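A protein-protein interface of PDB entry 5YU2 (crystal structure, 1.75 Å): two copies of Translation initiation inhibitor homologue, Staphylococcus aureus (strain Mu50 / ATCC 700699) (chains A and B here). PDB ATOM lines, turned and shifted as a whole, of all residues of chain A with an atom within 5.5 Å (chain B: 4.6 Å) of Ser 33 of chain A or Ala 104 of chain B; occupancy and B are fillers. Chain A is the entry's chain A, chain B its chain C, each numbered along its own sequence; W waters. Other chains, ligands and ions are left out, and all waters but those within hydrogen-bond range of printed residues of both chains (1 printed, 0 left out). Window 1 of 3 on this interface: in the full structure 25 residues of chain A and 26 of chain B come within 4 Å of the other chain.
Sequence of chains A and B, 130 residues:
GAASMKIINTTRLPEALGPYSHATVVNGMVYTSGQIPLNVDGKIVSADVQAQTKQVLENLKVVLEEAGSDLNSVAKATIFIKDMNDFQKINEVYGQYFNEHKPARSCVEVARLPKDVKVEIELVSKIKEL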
ATOM      1  N   TYR A  20     -10.958 -13.417 -16.482  1.00  0.00           N
ATOM      2  CA  TYR A  20     -10.704 -14.484 -17.432  1.00  0.00           C
ATOM      3  C   TYR A  20     -10.096 -15.699 -16.794  1.00  0.00           C
ATOM      4  O   TYR A  20      -9.697 -15.675 -15.611  1.00  0.00           O
ATOM      5  CB  TYR A  20      -9.856 -13.967 -18.567  1.00  0.00           C
ATOM      6  CG  TYR A  20      -8.396 -13.809 -18.329  1.00  0.00           C
ATOM      7  CD1 TYR A  20      -7.904 -12.729 -17.564  1.00  0.00           C
ATOM      8  CD2 TYR A  20      -7.514 -14.629 -18.961  1.00  0.00           C
ATOM      9  CE1 TYR A  20      -6.531 -12.557 -17.372  1.00  0.00           C
ATOM     10  CE2 TYR A  20      -6.141 -14.468 -18.792  1.00  0.00           C
ATOM     11  CZ  TYR A  20      -5.663 -13.433 -18.006  1.00  0.00           C
ATOM     12  OH  TYR A  20      -4.313 -13.307 -17.850  1.00  0.00           O
ATOM     13  N   SER A  21     -10.025 -16.791 -17.549  1.00  0.00           N
ATOM     14  CA  SER A  21      -9.502 -18.033 -17.075  1.00  0.00           C
ATOM     15  C   SER A  21      -8.453 -18.580 -18.054  1.00  0.00           C
ATOM     16  O   SER A  21      -8.466 -18.262 -19.210  1.00  0.00           O
ATOM     17  CB  SER A  21     -10.553 -19.038 -16.891  1.00  0.00           C
ATOM     18  OG  SER A  21     -11.492 -18.730 -15.859  1.00  0.00           O
ATOM     19  N   HIS A  22      -7.587 -19.451 -17.551  1.00  0.00           N
ATOM     20  CA  HIS A  22      -6.529 -20.012 -18.406  1.00  0.00           C
ATOM     21  C   HIS A  22      -7.129 -20.733 -19.601  1.00  0.00           C
ATOM     22  O   HIS A  22      -6.566 -20.632 -20.721  1.00  0.00           O
ATOM     23  CB  HIS A  22      -5.654 -21.010 -17.619  1.00  0.00           C
ATOM     24  CG  HIS A  22      -4.764 -20.381 -16.635  1.00  0.00           C
ATOM     25  ND1 HIS A  22      -4.466 -20.995 -15.439  1.00  0.00           N
ATOM     26  CD2 HIS A  22      -4.161 -19.162 -16.603  1.00  0.00           C
ATOM     27  CE1 HIS A  22      -3.692 -20.192 -14.727  1.00  0.00           C
ATOM     28  NE2 HIS A  22      -3.449 -19.106 -15.415  1.00  0.00           N
ATOM     29  N   ALA A  23      -8.197 -21.525 -19.391  1.00  0.00           N
ATOM     30  CA  ALA A  23      -8.922 -22.143 -20.474  1.00  0.00           C
ATOM     31  C   ALA A  23     -10.351 -22.429 -20.118  1.00  0.00           C
ATOM     32  O   ALA A  23     -10.762 -22.357 -18.935  1.00  0.00           O
ATOM     33  CB  ALA A  23      -8.233 -23.428 -20.969  1.00  0.00           C
ATOM     34  N   THR A  24     -11.142 -22.747 -21.134  1.00  0.00           N
ATOM     35  CA  THR A  24     -12.437 -23.389 -20.885  1.00  0.00           C
ATOM     36  C   THR A  24     -12.513 -24.678 -21.701  1.00  0.00           C
ATOM     37  O   THR A  24     -11.877 -24.778 -22.704  1.00  0.00           O
ATOM     38  CB  THR A  24     -13.641 -22.503 -21.270  1.00  0.00           C
ATOM     39  OG1 THR A  24     -13.598 -22.157 -22.651  1.00  0.00           O
ATOM     40  CG2 THR A  24     -13.686 -21.283 -20.434  1.00  0.00           C
ATOM     41  N   TYR A  31     -10.592 -24.257 -25.289  1.00  0.00           N
ATOM     42  CA  TYR A  31     -10.304 -22.883 -25.760  1.00  0.00           C
ATOM     43  C   TYR A  31      -9.324 -22.286 -24.762  1.00  0.00           C
ATOM     44  O   TYR A  31      -9.690 -22.048 -23.625  1.00  0.00           O
ATOM     45  CB  TYR A  31     -11.575 -22.024 -25.791  1.00  0.00           C
ATOM     46  CG  TYR A  31     -12.632 -22.558 -26.762  1.00  0.00           C
ATOM     47  CD1 TYR A  31     -13.548 -23.568 -26.354  1.00  0.00           C
ATOM     48  CD2 TYR A  31     -12.670 -22.151 -28.098  1.00  0.00           C
ATOM     49  CE1 TYR A  31     -14.459 -24.115 -27.273  1.00  0.00           C
ATOM     50  CE2 TYR A  31     -13.612 -22.669 -28.979  1.00  0.00           C
ATOM     51  CZ  TYR A  31     -14.487 -23.642 -28.559  1.00  0.00           C
ATOM     52  OH  TYR A  31     -15.412 -24.243 -29.416  1.00  0.00           O
ATOM     53  N   THR A  32      -8.081 -22.081 -25.165  1.00  0.00           N
ATOM     54  CA  THR A  32      -7.132 -21.448 -24.260  1.00  0.00           C
ATOM     55  C   THR A  32      -7.251 -19.950 -24.356  1.00  0.00           C
ATOM     56  O   THR A  32      -7.561 -19.406 -25.464  1.00  0.00           O
ATOM     57  CB  THR A  32      -5.667 -21.821 -24.497  1.00  0.00           C
ATOM     58  OG1 THR A  32      -5.083 -21.084 -25.608  1.00  0.00           O
ATOM     59  CG2 THR A  32      -5.561 -23.244 -24.726  1.00  0.00           C
ATOM     60  N   SER A  33      -6.952 -19.270 -23.239  1.00  0.00           N
ATOM     61  CA  SER A  33      -6.609 -17.823 -23.389  1.00  0.00           C
ATOM     62  C   SER A  33      -5.302 -17.678 -24.120  1.00  0.00           C
ATOM     63  O   SER A  33      -4.461 -18.645 -24.163  1.00  0.00           O
ATOM     64  CB  SER A  33      -6.523 -17.147 -22.010  1.00  0.00           C
ATOM     65  OG  SER A  33      -7.763 -17.050 -21.412  1.00  0.00           O
ATOM     66  N   GLY A  34      -5.059 -16.514 -24.748  1.00  0.00           N
ATOM     67  CA  GLY A  34      -3.773 -16.275 -25.323  1.00  0.00           C
ATOM     68  C   GLY A  34      -2.691 -16.324 -24.240  1.00  0.00           C
ATOM     69  O   GLY A  34      -2.883 -15.705 -23.142  1.00  0.00           O
ATOM     70  N   GLN A  35      -1.597 -17.004 -24.493  1.00  0.00           N
ATOM     71  CA  GLN A  35      -0.479 -17.008 -23.581  1.00  0.00           C
ATOM     72  C   GLN A  35       0.575 -16.066 -24.021  1.00  0.00           C
ATOM     73  O   GLN A  35       0.965 -16.068 -25.188  1.00  0.00           O
ATOM     74  CB  GLN A  35       0.140 -18.408 -23.406  1.00  0.00           C
ATOM     75  CG  GLN A  35      -0.676 -19.318 -22.429  1.00  0.00           C
ATOM     76  CD  GLN A  35      -0.496 -18.860 -20.980  1.00  0.00           C
ATOM     77  OE1 GLN A  35       0.570 -18.307 -20.640  1.00  0.00           O
ATOM     78  NE2 GLN A  35      -1.567 -18.891 -20.176  1.00  0.00           N
ATOM     79  N   LEU A  60       1.381 -23.051 -22.734  1.00  0.00           N
ATOM     80  CA  LEU A  60       0.260 -23.641 -23.381  1.00  0.00           C
ATOM     81  C   LEU A  60       0.249 -25.150 -23.155  1.00  0.00           C
ATOM     82  O   LEU A  60      -0.828 -25.714 -23.004  1.00  0.00           O
ATOM     83  CB  LEU A  60       0.247 -23.325 -24.903  1.00  0.00           C
ATOM     84  CG  LEU A  60      -0.112 -21.881 -25.195  1.00  0.00           C
ATOM     85  CD1 LEU A  60       0.261 -21.528 -26.601  1.00  0.00           C
ATOM     86  CD2 LEU A  60      -1.610 -21.668 -24.971  1.00  0.00           C
ATOM     87  N   ILE A 121       0.282 -16.569 -28.212  1.00  0.00           N
ATOM     88  CA  ILE A 121      -0.330 -17.673 -28.953  1.00  0.00           C
ATOM     89  C   ILE A 121      -1.560 -18.192 -28.254  1.00  0.00           C
ATOM     90  O   ILE A 121      -1.557 -18.388 -27.007  1.00  0.00           O
ATOM     91  CB  ILE A 121       0.666 -18.801 -29.243  1.00  0.00           C
ATOM     92  CG1 ILE A 121       1.828 -18.326 -30.050  1.00  0.00           C
ATOM     93  CG2 ILE A 121      -0.030 -19.957 -29.960  1.00  0.00           C
ATOM     94  CD1 ILE A 121       2.967 -19.319 -30.278  1.00  0.00           C
ATOM     95  N   GLU A 122      -2.636 -18.412 -29.006  1.00  0.00           N
ATOM     96  CA  GLU A 122      -3.820 -19.051 -28.475  1.00  0.00           C
ATOM     97  C   GLU A 122      -4.110 -20.313 -29.249  1.00  0.00           C
ATOM     98  O   GLU A 122      -3.762 -20.389 -30.442  1.00  0.00           O
ATOM     99  CB  GLU A 122      -5.085 -18.138 -28.443  1.00  0.00           C
ATOM    100  CG  GLU A 122      -5.412 -17.617 -29.861  1.00  0.00           C
ATOM    101  CD  GLU A 122      -6.674 -16.791 -29.929  1.00  0.00           C
ATOM    102  OE1 GLU A 122      -7.108 -16.164 -28.953  1.00  0.00           O
ATOM    103  OE2 GLU A 122      -7.258 -16.824 -30.993  1.00  0.00           O
ATOM    104  N   LEU A 123      -4.805 -21.244 -28.579  1.00  0.00           N
ATOM    105  CA  LEU A 123      -5.114 -22.538 -29.193  1.00  0.00           C
ATOM    106  C   LEU A 123      -6.539 -22.936 -28.968  1.00  0.00           C
ATOM    107  O   LEU A 123      -7.186 -22.589 -28.003  1.00  0.00           O
ATOM    108  CB  LEU A 123      -4.231 -23.686 -28.667  1.00  0.00           C
ATOM    109  CG  LEU A 123      -2.745 -23.515 -28.611  1.00  0.00           C
ATOM    110  CD1 LEU A 123      -2.044 -24.616 -27.820  1.00  0.00           C
ATOM    111  CD2 LEU A 123      -2.087 -23.260 -29.930  1.00  0.00           C
ATOM    112  N   ALA B  75     -17.593 -19.411 -23.994  1.00  0.00           N
ATOM    113  CA  ALA B  75     -16.367 -20.148 -23.919  1.00  0.00           C
ATOM    114  C   ALA B  75     -15.099 -19.282 -24.072  1.00  0.00           C
ATOM    115  O   ALA B  75     -14.066 -19.513 -23.388  1.00  0.00           O
ATOM    116  CB  ALA B  75     -16.378 -21.106 -25.043  1.00  0.00           C
ATOM    117  N   LYS B  76     -15.154 -18.335 -25.016  1.00  0.00           N
ATOM    118  CA  LYS B  76     -13.983 -17.606 -25.441  1.00  0.00           C
ATOM    119  C   LYS B  76     -14.357 -16.291 -26.000  1.00  0.00           C
ATOM    120  O   LYS B  76     -15.314 -16.144 -26.801  1.00  0.00           O
ATOM    121  CB  LYS B  76     -13.207 -18.399 -26.518  1.00  0.00           C
ATOM    122  CG  LYS B  76     -12.044 -17.723 -27.273  1.00  0.00           C
ATOM    123  CD  LYS B  76     -10.881 -17.566 -26.321  1.00  0.00           C
ATOM    124  CE  LYS B  76      -9.556 -17.215 -26.977  1.00  0.00           C
ATOM    125  NZ  LYS B  76      -9.714 -16.432 -28.171  1.00  0.00           N
ATOM    126  N   ALA B  77     -13.580 -15.281 -25.604  1.00  0.00           N
ATOM    127  CA  ALA B  77     -13.688 -13.951 -26.170  1.00  0.00           C
ATOM    128  C   ALA B  77     -12.368 -13.522 -26.802  1.00  0.00           C
ATOM    129  O   ALA B  77     -11.278 -13.845 -26.281  1.00  0.00           O
ATOM    130  CB  ALA B  77     -13.973 -12.934 -25.037  1.00  0.00           C
ATOM    131  N   LYS B 102     -15.975 -16.420 -16.084  1.00  0.00           N
ATOM    132  CA  LYS B 102     -14.691 -15.973 -16.591  1.00  0.00           C
ATOM    133  C   LYS B 102     -14.140 -16.822 -17.731  1.00  0.00           C
ATOM    134  O   LYS B 102     -13.392 -17.781 -17.539  1.00  0.00           O
ATOM    135  CB  LYS B 102     -13.698 -15.874 -15.455  1.00  0.00           C
ATOM    136  CG  LYS B 102     -14.107 -14.657 -14.603  1.00  0.00           C
ATOM    137  CD  LYS B 102     -13.212 -14.488 -13.438  1.00  0.00           C
ATOM    138  CE  LYS B 102     -13.777 -13.417 -12.535  1.00  0.00           C
ATOM    139  NZ  LYS B 102     -13.175 -13.652 -11.187  1.00  0.00           N
ATOM    140  N   PRO B 103     -14.580 -16.451 -18.928  1.00  0.00           N
ATOM    141  CA  PRO B 103     -14.195 -17.278 -20.059  1.00  0.00           C
ATOM    142  C   PRO B 103     -12.713 -17.117 -20.420  1.00  0.00           C
ATOM    143  O   PRO B 103     -11.992 -16.289 -19.936  1.00  0.00           O
ATOM    144  CB  PRO B 103     -15.025 -16.711 -21.188  1.00  0.00           C
ATOM    145  CG  PRO B 103     -15.555 -15.438 -20.791  1.00  0.00           C
ATOM    146  CD  PRO B 103     -15.456 -15.330 -19.305  1.00  0.00           C
ATOM    147  N   ALA B 104     -12.282 -17.941 -21.338  1.00  0.00           N
ATOM    148  CA  ALA B 104     -10.995 -17.713 -21.947  1.00  0.00           C
ATOM    149  C   ALA B 104     -11.018 -16.429 -22.791  1.00  0.00           C
ATOM    150  O   ALA B 104     -12.053 -16.068 -23.336  1.00  0.00           O
ATOM    151  CB  ALA B 104     -10.657 -18.905 -22.820  1.00  0.00           C
ATOM    152  N   ARG B 105      -9.877 -15.822 -22.949  1.00  0.00           N
ATOM    153  CA  ARG B 105      -9.782 -14.572 -23.686  1.00  0.00           C
ATOM    154  C   ARG B 105      -8.444 -14.348 -24.282  1.00  0.00           C
ATOM    155  O   ARG B 105      -7.419 -14.790 -23.752  1.00  0.00           O
ATOM    156  CB  ARG B 105     -10.123 -13.468 -22.672  1.00  0.00           C
ATOM    157  CG  ARG B 105      -9.964 -12.081 -23.013  1.00  0.00           C
ATOM    158  CD  ARG B 105     -10.234 -11.211 -21.758  1.00  0.00           C
ATOM    159  NE  ARG B 105      -9.060 -10.919 -20.974  1.00  0.00           N
ATOM    160  CZ  ARG B 105      -9.064  -9.991 -19.994  1.00  0.00           C
ATOM    161  NH1 ARG B 105     -10.144  -9.313 -19.711  1.00  0.00           N
ATOM    162  NH2 ARG B 105      -7.975  -9.750 -19.290  1.00  0.00           N
ATOM    163  N   SER B 106      -8.412 -13.615 -25.382  1.00  0.00           N
ATOM    164  CA  SER B 106      -7.219 -12.923 -25.856  1.00  0.00           C
ATOM    165  C   SER B 106      -7.511 -11.485 -26.164  1.00  0.00           C
ATOM    166  O   SER B 106      -8.646 -11.119 -26.496  1.00  0.00           O
ATOM    167  CB  SER B 106      -6.662 -13.582 -27.095  1.00  0.00           C
ATOM    168  OG  SER B 106      -6.410 -14.949 -26.867  1.00  0.00           O
HETATM  169  O   HOH W   1      -4.905 -13.618 -22.727  1.00  0.00           O
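The side-chain carboxylate of Glu 122 of chain A is in salt-bridge range of the side-chain amino group of Lys 76 of chain B (2.7 Å). The side-chain hydroxyl (OG) of Ser 33 of chain A lies within hydrogen-bond range of the backbone NH (N) of Arg 105 of chain B (2.9 Å). The backbone NH of Gly 34 of chain A lies within hydrogen-bond range of the backbone carbonyl oxygen of Arg 105 of chain B, at 3.1 Å. OG of Ser 106 of chain B is in hydrogen-bond range of N of Gly 34 of chain A (3.0 Å). OG of Ser 21 of chain A lies within hydrogen-bond range of O of Lys 102 of chain B (2.7 Å). The side-chain carboxylate of Glu 122 of chain A lies within hydrogen-bond range of the side-chain hydroxyl of Ser 106 of chain B (2.5 Å). OG1 of Thr 24 of chain A lies within hydrogen-bond range of O of Ala 75 of chain B (2.8 Å). N of Ser 21 of chain A lies within hydrogen-bond range of O of Pro 103 of chain B (3.1 Å).
The backbone carbonyl oxygen (O) of Thr 24 of chain A sits at hydrogen-bond distance from the backbone NH (N) of Tyr 31 of chain A, at 2.9 Å. O of Ser 21 of chain A lies within hydrogen-bond range of OG of Ser 33 of chain A (2.6 Å). The backbone carbonyl oxygen of Ala 77 of chain B lies within hydrogen-bond range of the backbone NH of Ser 106 of chain B, at 3.0 Å. The side-chain hydroxyl (OG1) of Thr 32 of chain A lies within hydrogen-bond range of the backbone NH (N) of Leu 123 of chain A (3.0 Å). O of Ala 75 of chain B sits at hydrogen-bond distance from N of Ala 104 of chain B. The backbone NH (N) of Ala 77 of chain B sits at hydrogen-bond distance from the backbone carbonyl oxygen (O) of Ala 104 of chain B, 2.8 Å away.
Among the printed residues, pairs that only touch across the chains: Thr 32 of chain A with Lys 76 of chain B (3.3 Å), Ser 33 of chain A with Ala 104 of chain B (3.3 Å), Tyr 20 of chain A with Pro 103 of chain B (3.3 Å), Tyr 31 of chain A with Ala 104 of chain B (3.4 Å), Tyr 20 of chain A with Arg 105 of chain B (3.4 Å), Thr 24 of chain A with Ala 104 of chain B (3.7 Å), Ser 21 of chain A with Ala 104 of chain B (3.8 Å), Tyr 20 of chain A with Lys 102 of chain B (3.8 Å), Thr 32 of chain A with Ala 104 of chain B (3.9 Å) and Tyr 31 of chain A with Ala 75 of chain B (3.97 Å).
Ser 33 of chain A touches just these residues of chain B: Ala 104 (3.3 Å) and Arg 105 (2.9 Å). Of the printed residues of chain B, Glu 122 of chain A touches Lys 76 (2.7 Å) and Ser 106 (2.5 Å). Printed residues of chain A within 4 Å of Lys 76 of chain B: Thr 32 and Glu 122. Of the printed residues of chain A, Pro 103 of chain B touches Tyr 20 and Ser 21. Ala 104 of chain B touches just these residues of chain A: Ser 21, Thr 24, Tyr 31, Thr 32 and Ser 33. Of the printed residues of chain A, Ser 106 of chain B touches Gly 34 (3.0 Å) and Glu 122 (2.5 Å). The nearest residue of chain B that does not touch Ser 33 of chain A is Ser 106 of chain B (4.03 Å).
Of the 8 printed residues of chain B, 7 touch a printed residue of chain A. Hydrophobic or aromatic side chains of chain B within 4 Å of the printed part of chain A: Ala 75 and Ala 104. Of the 14 printed residues of chain A, 8 touch a printed residue of chain B. Printed residues of chain A that touch a printed residue of chain B: Tyr 20, Ser 21, Thr 24, Tyr 31, Thr 32, Ser 33, Gly 34 and Glu 122. Hydrophobic or aromatic side chains of chain A within 4 Å of the printed part of chain B: Tyr 20 and Tyr 31. Among the printed residues, Asp or Glu carboxylates within 4 Å of a Lys or Arg side-chain nitrogen of the other chain: Glu 122 of chain A with Lys 76 of chain B (2.7 Å).
No position is printed for both chains.
Water W1 bridges O of Gly 34 of chain A (2.9 Å) and O of Arg 105 of chain B (3.0 Å).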
